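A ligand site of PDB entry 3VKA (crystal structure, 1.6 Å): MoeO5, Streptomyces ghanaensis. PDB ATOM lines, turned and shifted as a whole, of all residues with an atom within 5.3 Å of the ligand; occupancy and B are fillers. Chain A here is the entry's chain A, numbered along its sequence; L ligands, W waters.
An oxygen (O4) of the ligand sits at hydrogen-bond distance from the side-chain hydroxyl of Ser 233 (2.6 Å). The backbone NH (N) of Gly 257 sits at hydrogen-bond distance from an oxygen (O5) of the ligand (2.8 Å). O3 of the ligand lies within hydrogen-bond range of N of Ala 256, at 2.8 Å. The backbone NH (N) of Asn 235 sits at hydrogen-bond distance from an oxygen (O7) of the ligand (2.7 Å). The side-chain hydroxyl of Tyr 204 sits at hydrogen-bond distance from an oxygen (O4) of the ligand (2.4 Å).
OG1 of Thr 75 sits at hydrogen-bond distance from NH2 of Arg 208, at 3.0 Å. The backbone NH (N) of Tyr 206 is in hydrogen-bond range of the backbone carbonyl oxygen (O) of Leu 163, 2.9 Å away. NH1 of Arg 208 sits close to OH of Tyr 206, 3.3 Å away. O of Phe 255 is in hydrogen-bond range of N of Ile 44 (2.9 Å). The backbone carbonyl oxygen of Tyr 204 is in hydrogen-bond range of the backbone NH of Leu 163 (3.0 Å). The side-chain hydroxyl (OH) of Tyr 204 sits at hydrogen-bond distance from the side-chain hydroxyl (OG) of Ser 233, at 3.1 Å. O of Ser 207 lies within hydrogen-bond range of ND2 of Asn 235, 3.4 Å away. The backbone carbonyl oxygen (O) of His 102 lies within hydrogen-bond range of the backbone NH (N) of Ser 74 (3.4 Å).
Merely in contact with the ligand: Ile 44, Ala 73, Ser 74, Thr 75, His 102, Pro 104, Pro 123, Leu 125, Ala 162, Thr 164, Leu 175, Tyr 206, Gly 234 and Phe 255. Hydrophobic or aromatic side chains within 4 Å of the ligand: Ile 44, Ala 73, His 102, Pro 104, Pro 123, Leu 125, Ala 162, Leu 175, Tyr 204, Tyr 206 and Ala 256. Within 4 Å of the ligand: Ile 44, Ala 73, Ser 74, Thr 75, His 102, Pro 104, Pro 123, Leu 125, Ala 162, Thr 164, Leu 175, Tyr 204, Tyr 206, Ser 233, Gly 234, Asn 235, Phe 255, Ala 256 and Gly 257. Along chain A the residues within 4 Å of the ligand span positions 44 to 257. The nearest printed residue that does not touch the ligand is Phe 103 (4.04 Å).
Water W1 lies within hydrogen-bond range of the backbone carbonyl oxygen of Arg 208 (2.7 Å) and an oxygen (O7) of the ligand (2.7 Å). Water W2 lies within hydrogen-bond range of the backbone carbonyl oxygen of Val 236 (2.8 Å), an oxygen (O3) of the ligand (2.8 Å), the backbone NH of Ala 258 (3.0 Å) and the backbone NH of Gly 257 (3.4 Å). Water W7 lies within hydrogen-bond range of OH of Tyr 206 and O2 of the ligand. Water W6 lies within hydrogen-bond range of OH of Tyr 204 (2.9 Å), ND1 of His 102 (2.9 Å) and O6 of the ligand (2.9 Å). Water W4 lies within hydrogen-bond range of the backbone carbonyl oxygen of Ala 73 (2.9 Å) and an oxygen (O6) of the ligand (3.0 Å).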
ATOM      1  N   ILE A  44       9.883 -11.069  -5.774  1.00  0.00           N
ATOM      2  CA  ILE A  44       9.181 -12.256  -6.227  1.00  0.00           C
ATOM      3  C   ILE A  44      10.180 -13.410  -6.092  1.00  0.00           C
ATOM      4  O   ILE A  44      11.233 -13.404  -6.720  1.00  0.00           O
ATOM      5  CB  ILE A  44       8.770 -12.072  -7.675  1.00  0.00           C
ATOM      6  CG1 ILE A  44       7.782 -10.920  -7.753  1.00  0.00           C
ATOM      7  CG2 ILE A  44       8.132 -13.376  -8.161  1.00  0.00           C
ATOM      8  CD1 ILE A  44       7.684 -10.355  -9.169  1.00  0.00           C
ATOM      9  N   ALA A  73       6.251 -16.951  -7.387  1.00  0.00           N
ATOM     10  CA  ALA A  73       5.785 -17.045  -8.779  1.00  0.00           C
ATOM     11  C   ALA A  73       6.768 -17.722  -9.676  1.00  0.00           C
ATOM     12  O   ALA A  73       7.974 -17.605  -9.486  1.00  0.00           O
ATOM     13  CB  ALA A  73       5.532 -15.580  -9.312  1.00  0.00           C
ATOM     14  N   SER A  74       6.238 -18.407 -10.700  1.00  0.00           N
ATOM     15  CA  SER A  74       7.124 -19.039 -11.680  1.00  0.00           C
ATOM     16  C   SER A  74       6.292 -19.325 -12.894  1.00  0.00           C
ATOM     17  O   SER A  74       5.086 -19.538 -12.801  1.00  0.00           O
ATOM     18  CB  SER A  74       7.635 -20.390 -11.156  1.00  0.00           C
ATOM     19  OG  SER A  74       8.566 -20.946 -12.104  1.00  0.00           O
ATOM     20  N   THR A  75       6.968 -19.347 -14.042  1.00  0.00           N
ATOM     21  CA  THR A  75       6.267 -19.737 -15.258  1.00  0.00           C
ATOM     22  C   THR A  75       6.115 -21.271 -15.264  1.00  0.00           C
ATOM     23  O   THR A  75       5.146 -21.843 -15.800  1.00  0.00           O
ATOM     24  CB  THR A  75       7.120 -19.307 -16.479  1.00  0.00           C
ATOM     25  OG1 THR A  75       7.192 -17.865 -16.539  1.00  0.00           O
ATOM     26  CG2 THR A  75       6.527 -19.883 -17.729  1.00  0.00           C
ATOM     27  N   HIS A 102       1.537 -16.657  -7.765  1.00  0.00           N
ATOM     28  CA  HIS A 102       1.232 -16.200  -9.169  1.00  0.00           C
ATOM     29  C   HIS A 102       1.856 -17.192 -10.165  1.00  0.00           C
ATOM     30  O   HIS A 102       3.108 -17.240 -10.359  1.00  0.00           O
ATOM     31  CB  HIS A 102       1.782 -14.805  -9.413  1.00  0.00           C
ATOM     32  CG  HIS A 102       1.412 -14.250 -10.751  1.00  0.00           C
ATOM     33  ND1 HIS A 102       2.134 -13.239 -11.351  1.00  0.00           N
ATOM     34  CD2 HIS A 102       0.367 -14.531 -11.578  1.00  0.00           C
ATOM     35  CE1 HIS A 102       1.531 -12.916 -12.501  1.00  0.00           C
ATOM     36  NE2 HIS A 102       0.462 -13.677 -12.658  1.00  0.00           N
ATOM     37  N   PHE A 103       0.984 -18.002 -10.785  1.00  0.00           N
ATOM     38  CA  PHE A 103       1.417 -19.048 -11.696  1.00  0.00           C
ATOM     39  C   PHE A 103       0.381 -19.142 -12.835  1.00  0.00           C
ATOM     40  O   PHE A 103      -0.781 -18.783 -12.651  1.00  0.00           O
ATOM     41  CB  PHE A 103       1.431 -20.429 -10.990  1.00  0.00           C
ATOM     42  CG  PHE A 103       2.414 -20.495  -9.838  1.00  0.00           C
ATOM     43  CD1 PHE A 103       2.020 -20.059  -8.581  1.00  0.00           C
ATOM     44  CD2 PHE A 103       3.732 -20.899 -10.059  1.00  0.00           C
ATOM     45  CE1 PHE A 103       2.948 -20.040  -7.528  1.00  0.00           C
ATOM     46  CE2 PHE A 103       4.666 -20.880  -9.030  1.00  0.00           C
ATOM     47  CZ  PHE A 103       4.254 -20.438  -7.752  1.00  0.00           C
ATOM     48  N   PRO A 104       0.812 -19.620 -13.992  1.00  0.00           N
ATOM     49  CA  PRO A 104      -0.157 -19.755 -15.092  1.00  0.00           C
ATOM     50  C   PRO A 104      -1.070 -20.954 -14.838  1.00  0.00           C
ATOM     51  O   PRO A 104      -0.725 -21.905 -14.129  1.00  0.00           O
ATOM     52  CB  PRO A 104       0.716 -20.003 -16.330  1.00  0.00           C
ATOM     53  CG  PRO A 104       1.970 -20.662 -15.784  1.00  0.00           C
ATOM     54  CD  PRO A 104       2.187 -19.999 -14.371  1.00  0.00           C
ATOM     55  N   PRO A 123      -4.206 -14.119 -13.333  1.00  0.00           N
ATOM     56  CA  PRO A 123      -3.964 -13.277 -14.513  1.00  0.00           C
ATOM     57  C   PRO A 123      -4.929 -13.613 -15.663  1.00  0.00           C
ATOM     58  O   PRO A 123      -4.959 -14.796 -16.106  1.00  0.00           O
ATOM     59  CB  PRO A 123      -2.522 -13.631 -14.901  1.00  0.00           C
ATOM     60  CG  PRO A 123      -2.317 -15.109 -14.413  1.00  0.00           C
ATOM     61  CD  PRO A 123      -3.094 -15.079 -13.088  1.00  0.00           C
ATOM     62  N   LEU A 125      -5.140 -13.015 -19.347  1.00  0.00           N
ATOM     63  CA  LEU A 125      -4.158 -12.596 -20.392  1.00  0.00           C
ATOM     64  C   LEU A 125      -4.927 -12.053 -21.566  1.00  0.00           C
ATOM     65  O   LEU A 125      -5.182 -12.757 -22.573  1.00  0.00           O
ATOM     66  CB  LEU A 125      -3.268 -13.826 -20.720  1.00  0.00           C
ATOM     67  CG  LEU A 125      -2.388 -14.153 -19.481  1.00  0.00           C
ATOM     68  CD1 LEU A 125      -2.069 -15.636 -19.416  1.00  0.00           C
ATOM     69  CD2 LEU A 125      -1.099 -13.343 -19.478  1.00  0.00           C
ATOM     70  N   ALA A 162      -3.481  -9.119 -17.097  1.00  0.00           N
ATOM     71  CA  ALA A 162      -2.071  -9.366 -17.288  1.00  0.00           C
ATOM     72  C   ALA A 162      -1.703  -9.178 -18.716  1.00  0.00           C
ATOM     73  O   ALA A 162      -2.302  -9.823 -19.583  1.00  0.00           O
ATOM     74  CB  ALA A 162      -1.731 -10.821 -16.827  1.00  0.00           C
ATOM     75  N   LEU A 163      -0.707  -8.345 -18.913  1.00  0.00           N
ATOM     76  CA  LEU A 163      -0.275  -7.959 -20.262  1.00  0.00           C
ATOM     77  C   LEU A 163       1.210  -8.143 -20.439  1.00  0.00           C
ATOM     78  O   LEU A 163       2.000  -7.846 -19.536  1.00  0.00           O
ATOM     79  CB  LEU A 163      -0.690  -6.495 -20.468  1.00  0.00           C
ATOM     80  CG  LEU A 163      -2.196  -6.229 -20.323  1.00  0.00           C
ATOM     81  CD1 LEU A 163      -2.430  -4.720 -20.515  1.00  0.00           C
ATOM     82  CD2 LEU A 163      -2.978  -7.012 -21.404  1.00  0.00           C
ATOM     83  N   THR A 164       1.627  -8.520 -21.639  1.00  0.00           N
ATOM     84  CA  THR A 164       3.015  -8.772 -21.894  1.00  0.00           C
ATOM     85  C   THR A 164       3.568  -7.806 -22.911  1.00  0.00           C
ATOM     86  O   THR A 164       2.885  -7.431 -23.898  1.00  0.00           O
ATOM     87  CB  THR A 164       3.253 -10.241 -22.379  1.00  0.00           C
ATOM     88  OG1 THR A 164       2.662 -10.454 -23.670  1.00  0.00           O
ATOM     89  CG2 THR A 164       2.656 -11.242 -21.407  1.00  0.00           C
ATOM     90  N   THR A 171       6.375 -17.017 -23.388  1.00  0.00           N
ATOM     91  CA  THR A 171       4.995 -16.860 -22.965  1.00  0.00           C
ATOM     92  C   THR A 171       4.054 -17.019 -24.146  1.00  0.00           C
ATOM     93  O   THR A 171       2.954 -17.513 -24.023  1.00  0.00           O
ATOM     94  CB  THR A 171       4.750 -15.508 -22.300  1.00  0.00           C
ATOM     95  OG1 THR A 171       5.843 -15.232 -21.395  1.00  0.00           O
ATOM     96  CG2 THR A 171       3.438 -15.539 -21.540  1.00  0.00           C
ATOM     97  N   LEU A 175       1.267 -19.642 -23.474  1.00  0.00           N
ATOM     98  CA  LEU A 175      -0.019 -19.035 -23.127  1.00  0.00           C
ATOM     99  C   LEU A 175      -0.734 -18.313 -24.234  1.00  0.00           C
ATOM    100  O   LEU A 175      -1.831 -17.780 -24.038  1.00  0.00           O
ATOM    101  CB  LEU A 175       0.143 -18.058 -21.929  1.00  0.00           C
ATOM    102  CG  LEU A 175       1.002 -18.540 -20.774  1.00  0.00           C
ATOM    103  CD1 LEU A 175       1.079 -17.462 -19.715  1.00  0.00           C
ATOM    104  CD2 LEU A 175       0.410 -19.814 -20.168  1.00  0.00           C
ATOM    105  N   TYR A 204      -1.277  -6.099 -14.210  1.00  0.00           N
ATOM    106  CA  TYR A 204       0.100  -6.539 -14.108  1.00  0.00           C
ATOM    107  C   TYR A 204       0.708  -6.376 -15.489  1.00  0.00           C
ATOM    108  O   TYR A 204       0.286  -7.063 -16.442  1.00  0.00           O
ATOM    109  CB  TYR A 204       0.109  -8.010 -13.661  1.00  0.00           C
ATOM    110  CG  TYR A 204       1.432  -8.497 -13.091  1.00  0.00           C
ATOM    111  CD1 TYR A 204       2.562  -8.599 -13.897  1.00  0.00           C
ATOM    112  CD2 TYR A 204       1.535  -8.786 -11.725  1.00  0.00           C
ATOM    113  CE1 TYR A 204       3.787  -8.981 -13.363  1.00  0.00           C
ATOM    114  CE2 TYR A 204       2.753  -9.178 -11.185  1.00  0.00           C
ATOM    115  CZ  TYR A 204       3.860  -9.279 -12.000  1.00  0.00           C
ATOM    116  OH  TYR A 204       5.027  -9.703 -11.427  1.00  0.00           O
ATOM    117  N   TYR A 206       4.013  -6.818 -17.662  1.00  0.00           N
ATOM    118  CA  TYR A 206       5.217  -7.651 -17.576  1.00  0.00           C
ATOM    119  C   TYR A 206       6.031  -7.674 -18.864  1.00  0.00           C
ATOM    120  O   TYR A 206       5.443  -7.680 -19.960  1.00  0.00           O
ATOM    121  CB  TYR A 206       4.724  -9.090 -17.291  1.00  0.00           C
ATOM    122  CG  TYR A 206       5.762 -10.201 -17.448  1.00  0.00           C
ATOM    123  CD1 TYR A 206       6.845 -10.308 -16.559  1.00  0.00           C
ATOM    124  CD2 TYR A 206       5.621 -11.140 -18.451  1.00  0.00           C
ATOM    125  CE1 TYR A 206       7.775 -11.364 -16.689  1.00  0.00           C
ATOM    126  CE2 TYR A 206       6.521 -12.188 -18.571  1.00  0.00           C
ATOM    127  CZ  TYR A 206       7.580 -12.299 -17.701  1.00  0.00           C
ATOM    128  OH  TYR A 206       8.428 -13.388 -17.804  1.00  0.00           O
ATOM    129  N   SER A 207       7.375  -7.715 -18.739  1.00  0.00           N
ATOM    130  CA  SER A 207       8.209  -7.928 -19.935  1.00  0.00           C
ATOM    131  C   SER A 207       9.216  -9.018 -19.549  1.00  0.00           C
ATOM    132  O   SER A 207      10.072  -8.792 -18.683  1.00  0.00           O
ATOM    133  CB  SER A 207       8.960  -6.660 -20.370  1.00  0.00           C
ATOM    134  OG  SER A 207       9.649  -6.958 -21.585  1.00  0.00           O
ATOM    135  N   ARG A 208       9.162 -10.164 -20.240  1.00  0.00           N
ATOM    136  CA  ARG A 208      10.113 -11.228 -19.909  1.00  0.00           C
ATOM    137  C   ARG A 208      11.535 -10.850 -20.333  1.00  0.00           C
ATOM    138  O   ARG A 208      12.499 -11.066 -19.567  1.00  0.00           O
ATOM    139  CB  ARG A 208       9.717 -12.534 -20.637  1.00  0.00           C
ATOM    140  CG  ARG A 208      10.639 -13.683 -20.210  1.00  0.00           C
ATOM    141  CD  ARG A 208      10.254 -14.996 -20.889  1.00  0.00           C
ATOM    142  NE  ARG A 208       8.914 -15.460 -20.540  1.00  0.00           N
ATOM    143  CZ  ARG A 208       8.619 -16.130 -19.426  1.00  0.00           C
ATOM    144  NH1 ARG A 208       9.573 -16.409 -18.555  1.00  0.00           N
ATOM    145  NH2 ARG A 208       7.366 -16.481 -19.218  1.00  0.00           N
ATOM    146  N   SER A 233       6.623  -5.556 -13.774  1.00  0.00           N
ATOM    147  CA  SER A 233       7.809  -6.380 -13.508  1.00  0.00           C
ATOM    148  C   SER A 233       8.480  -6.782 -14.801  1.00  0.00           C
ATOM    149  O   SER A 233       7.915  -6.643 -15.922  1.00  0.00           O
ATOM    150  CB  SER A 233       7.498  -7.620 -12.651  1.00  0.00           C
ATOM    151  OG  SER A 233       7.077  -8.682 -13.455  1.00  0.00           O
ATOM    152  N   GLY A 234       9.726  -7.244 -14.650  1.00  0.00           N
ATOM    153  CA  GLY A 234      10.497  -7.726 -15.771  1.00  0.00           C
ATOM    154  C   GLY A 234      11.795  -6.970 -15.921  1.00  0.00           C
ATOM    155  O   GLY A 234      11.799  -5.790 -16.289  1.00  0.00           O
ATOM    156  N   ASN A 235      12.860  -7.679 -15.592  1.00  0.00           N
ATOM    157  CA  ASN A 235      14.182  -7.110 -15.734  1.00  0.00           C
ATOM    158  C   ASN A 235      14.486  -5.874 -14.957  1.00  0.00           C
ATOM    159  O   ASN A 235      15.239  -5.014 -15.420  1.00  0.00           O
ATOM    160  CB  ASN A 235      14.439  -6.916 -17.245  1.00  0.00           C
ATOM    161  CG  ASN A 235      14.397  -8.223 -17.963  1.00  0.00           C
ATOM    162  OD1 ASN A 235      15.157  -9.180 -17.614  1.00  0.00           O
ATOM    163  ND2 ASN A 235      13.463  -8.359 -18.882  1.00  0.00           N
ATOM    164  N   VAL A 236      13.885  -5.761 -13.765  1.00  0.00           N
ATOM    165  CA  VAL A 236      14.169  -4.650 -12.883  1.00  0.00           C
ATOM    166  C   VAL A 236      15.367  -5.069 -12.051  1.00  0.00           C
ATOM    167  O   VAL A 236      15.311  -6.052 -11.305  1.00  0.00           O
ATOM    168  CB  VAL A 236      12.991  -4.396 -11.984  1.00  0.00           C
ATOM    169  CG1 VAL A 236      13.365  -3.356 -10.865  1.00  0.00           C
ATOM    170  CG2 VAL A 236      11.808  -3.898 -12.827  1.00  0.00           C
ATOM    171  N   GLY A 254       7.864  -5.299  -9.315  1.00  0.00           N
ATOM    172  CA  GLY A 254       8.359  -6.624  -8.953  1.00  0.00           C
ATOM    173  C   GLY A 254       9.721  -6.949  -9.510  1.00  0.00           C
ATOM    174  O   GLY A 254      10.098  -6.445 -10.562  1.00  0.00           O
ATOM    175  N   PHE A 255      10.478  -7.774  -8.798  1.00  0.00           N
ATOM    176  CA  PHE A 255      11.799  -8.182  -9.270  1.00  0.00           C
ATOM    177  C   PHE A 255      12.112  -9.539  -8.653  1.00  0.00           C
ATOM    178  O   PHE A 255      11.831  -9.779  -7.459  1.00  0.00           O
ATOM    179  CB  PHE A 255      12.894  -7.150  -8.898  1.00  0.00           C
ATOM    180  CG  PHE A 255      13.067  -6.961  -7.391  1.00  0.00           C
ATOM    181  CD1 PHE A 255      12.135  -6.250  -6.679  1.00  0.00           C
ATOM    182  CD2 PHE A 255      14.188  -7.509  -6.743  1.00  0.00           C
ATOM    183  CE1 PHE A 255      12.297  -6.064  -5.283  1.00  0.00           C
ATOM    184  CE2 PHE A 255      14.349  -7.306  -5.334  1.00  0.00           C
ATOM    185  CZ  PHE A 255      13.435  -6.601  -4.644  1.00  0.00           C
ATOM    186  N   ALA A 256      12.573 -10.443  -9.508  1.00  0.00           N
ATOM    187  CA  ALA A 256      12.893 -11.815  -9.079  1.00  0.00           C
ATOM    188  C   ALA A 256      14.354 -12.110  -9.365  1.00  0.00           C
ATOM    189  O   ALA A 256      15.163 -12.241  -8.423  1.00  0.00           O
ATOM    190  CB  ALA A 256      12.011 -12.829  -9.816  1.00  0.00           C
ATOM    191  N   GLY A 257      14.720 -12.120 -10.660  1.00  0.00           N
ATOM    192  CA  GLY A 257      16.063 -12.500 -11.046  1.00  0.00           C
ATOM    193  C   GLY A 257      17.244 -11.804 -10.429  1.00  0.00           C
ATOM    194  O   GLY A 257      18.280 -12.424 -10.226  1.00  0.00           O
ATOM    195  N   ALA A 258      17.069 -10.536 -10.115  1.00  0.00           N
ATOM    196  CA  ALA A 258      18.158  -9.770  -9.538  1.00  0.00           C
ATOM    197  C   ALA A 258      18.650 -10.437  -8.255  1.00  0.00           C
ATOM    198  O   ALA A 258      19.822 -10.281  -7.887  1.00  0.00           O
ATOM    199  CB  ALA A 258      17.681  -8.341  -9.247  1.00  0.00           C
HETATM  200  P1  LIG L   1      12.471 -10.795 -13.309  1.00  0.00           P
HETATM  201  C1  LIG L   1       8.045 -14.498 -14.119  1.00  0.00           C
HETATM  202  C2  LIG L   1       6.807 -13.768 -14.626  1.00  0.00           C
HETATM  203  C3  LIG L   1       5.568 -13.931 -14.133  1.00  0.00           C
HETATM  204  C4  LIG L   1       4.575 -13.101 -14.777  1.00  0.00           C
HETATM  205  C5  LIG L   1       5.155 -14.889 -12.974  1.00  0.00           C
HETATM  206  C6  LIG L   1       4.628 -16.206 -13.590  1.00  0.00           C
HETATM  207  C7  LIG L   1       3.158 -16.110 -13.986  1.00  0.00           C
HETATM  208  C8  LIG L   1       2.689 -16.333 -15.249  1.00  0.00           C
HETATM  209  C9  LIG L   1       3.540 -16.698 -16.432  1.00  0.00           C
HETATM  210  C10 LIG L   1       9.788 -11.214 -12.812  1.00  0.00           C
HETATM  211  O1  LIG L   1      10.789 -11.334 -13.653  1.00  0.00           O
HETATM  212  C11 LIG L   1       8.708 -12.185 -13.208  1.00  0.00           C
HETATM  213  O2  LIG L   1       9.069 -13.538 -13.494  1.00  0.00           O
HETATM  214  C12 LIG L   1       7.583 -12.057 -12.199  1.00  0.00           C
HETATM  215  C13 LIG L   1       1.173 -16.197 -15.478  1.00  0.00           C
HETATM  216  C14 LIG L   1       0.746 -15.198 -16.562  1.00  0.00           C
HETATM  217  C15 LIG L   1       1.052 -13.800 -16.209  1.00  0.00           C
HETATM  218  C16 LIG L   1       1.770 -12.968 -16.927  1.00  0.00           C
HETATM  219  C17 LIG L   1       2.461 -13.331 -18.244  1.00  0.00           C
HETATM  220  C18 LIG L   1       1.933 -11.583 -16.368  1.00  0.00           C
HETATM  221  O3  LIG L   1      12.549  -9.775 -12.184  1.00  0.00           O
HETATM  222  O4  LIG L   1       6.901 -10.987 -12.262  1.00  0.00           O
HETATM  223  O5  LIG L   1      13.380 -11.986 -13.087  1.00  0.00           O
HETATM  224  O6  LIG L   1       7.351 -13.003 -11.421  1.00  0.00           O
HETATM  225  O7  LIG L   1      12.878 -10.227 -14.676  1.00  0.00           O
HETATM  226  O   HOH W   1      12.531 -11.761 -16.924  1.00  0.00           O
HETATM  227  O   HOH W   2      15.105  -8.792 -11.476  1.00  0.00           O
HETATM  228  O   HOH W   3      15.878  -9.722 -14.070  1.00  0.00           O
HETATM  229  O   HOH W   4       9.144 -15.306 -10.880  1.00  0.00           O
HETATM  230  O   HOH W   5      11.630  -7.372 -12.663  1.00  0.00           O
HETATM  231  O   HOH W   6       4.700 -12.345 -10.354  1.00  0.00           O
HETATM  232  O   HOH W   7      10.437 -13.593 -16.084  1.00  0.00           O
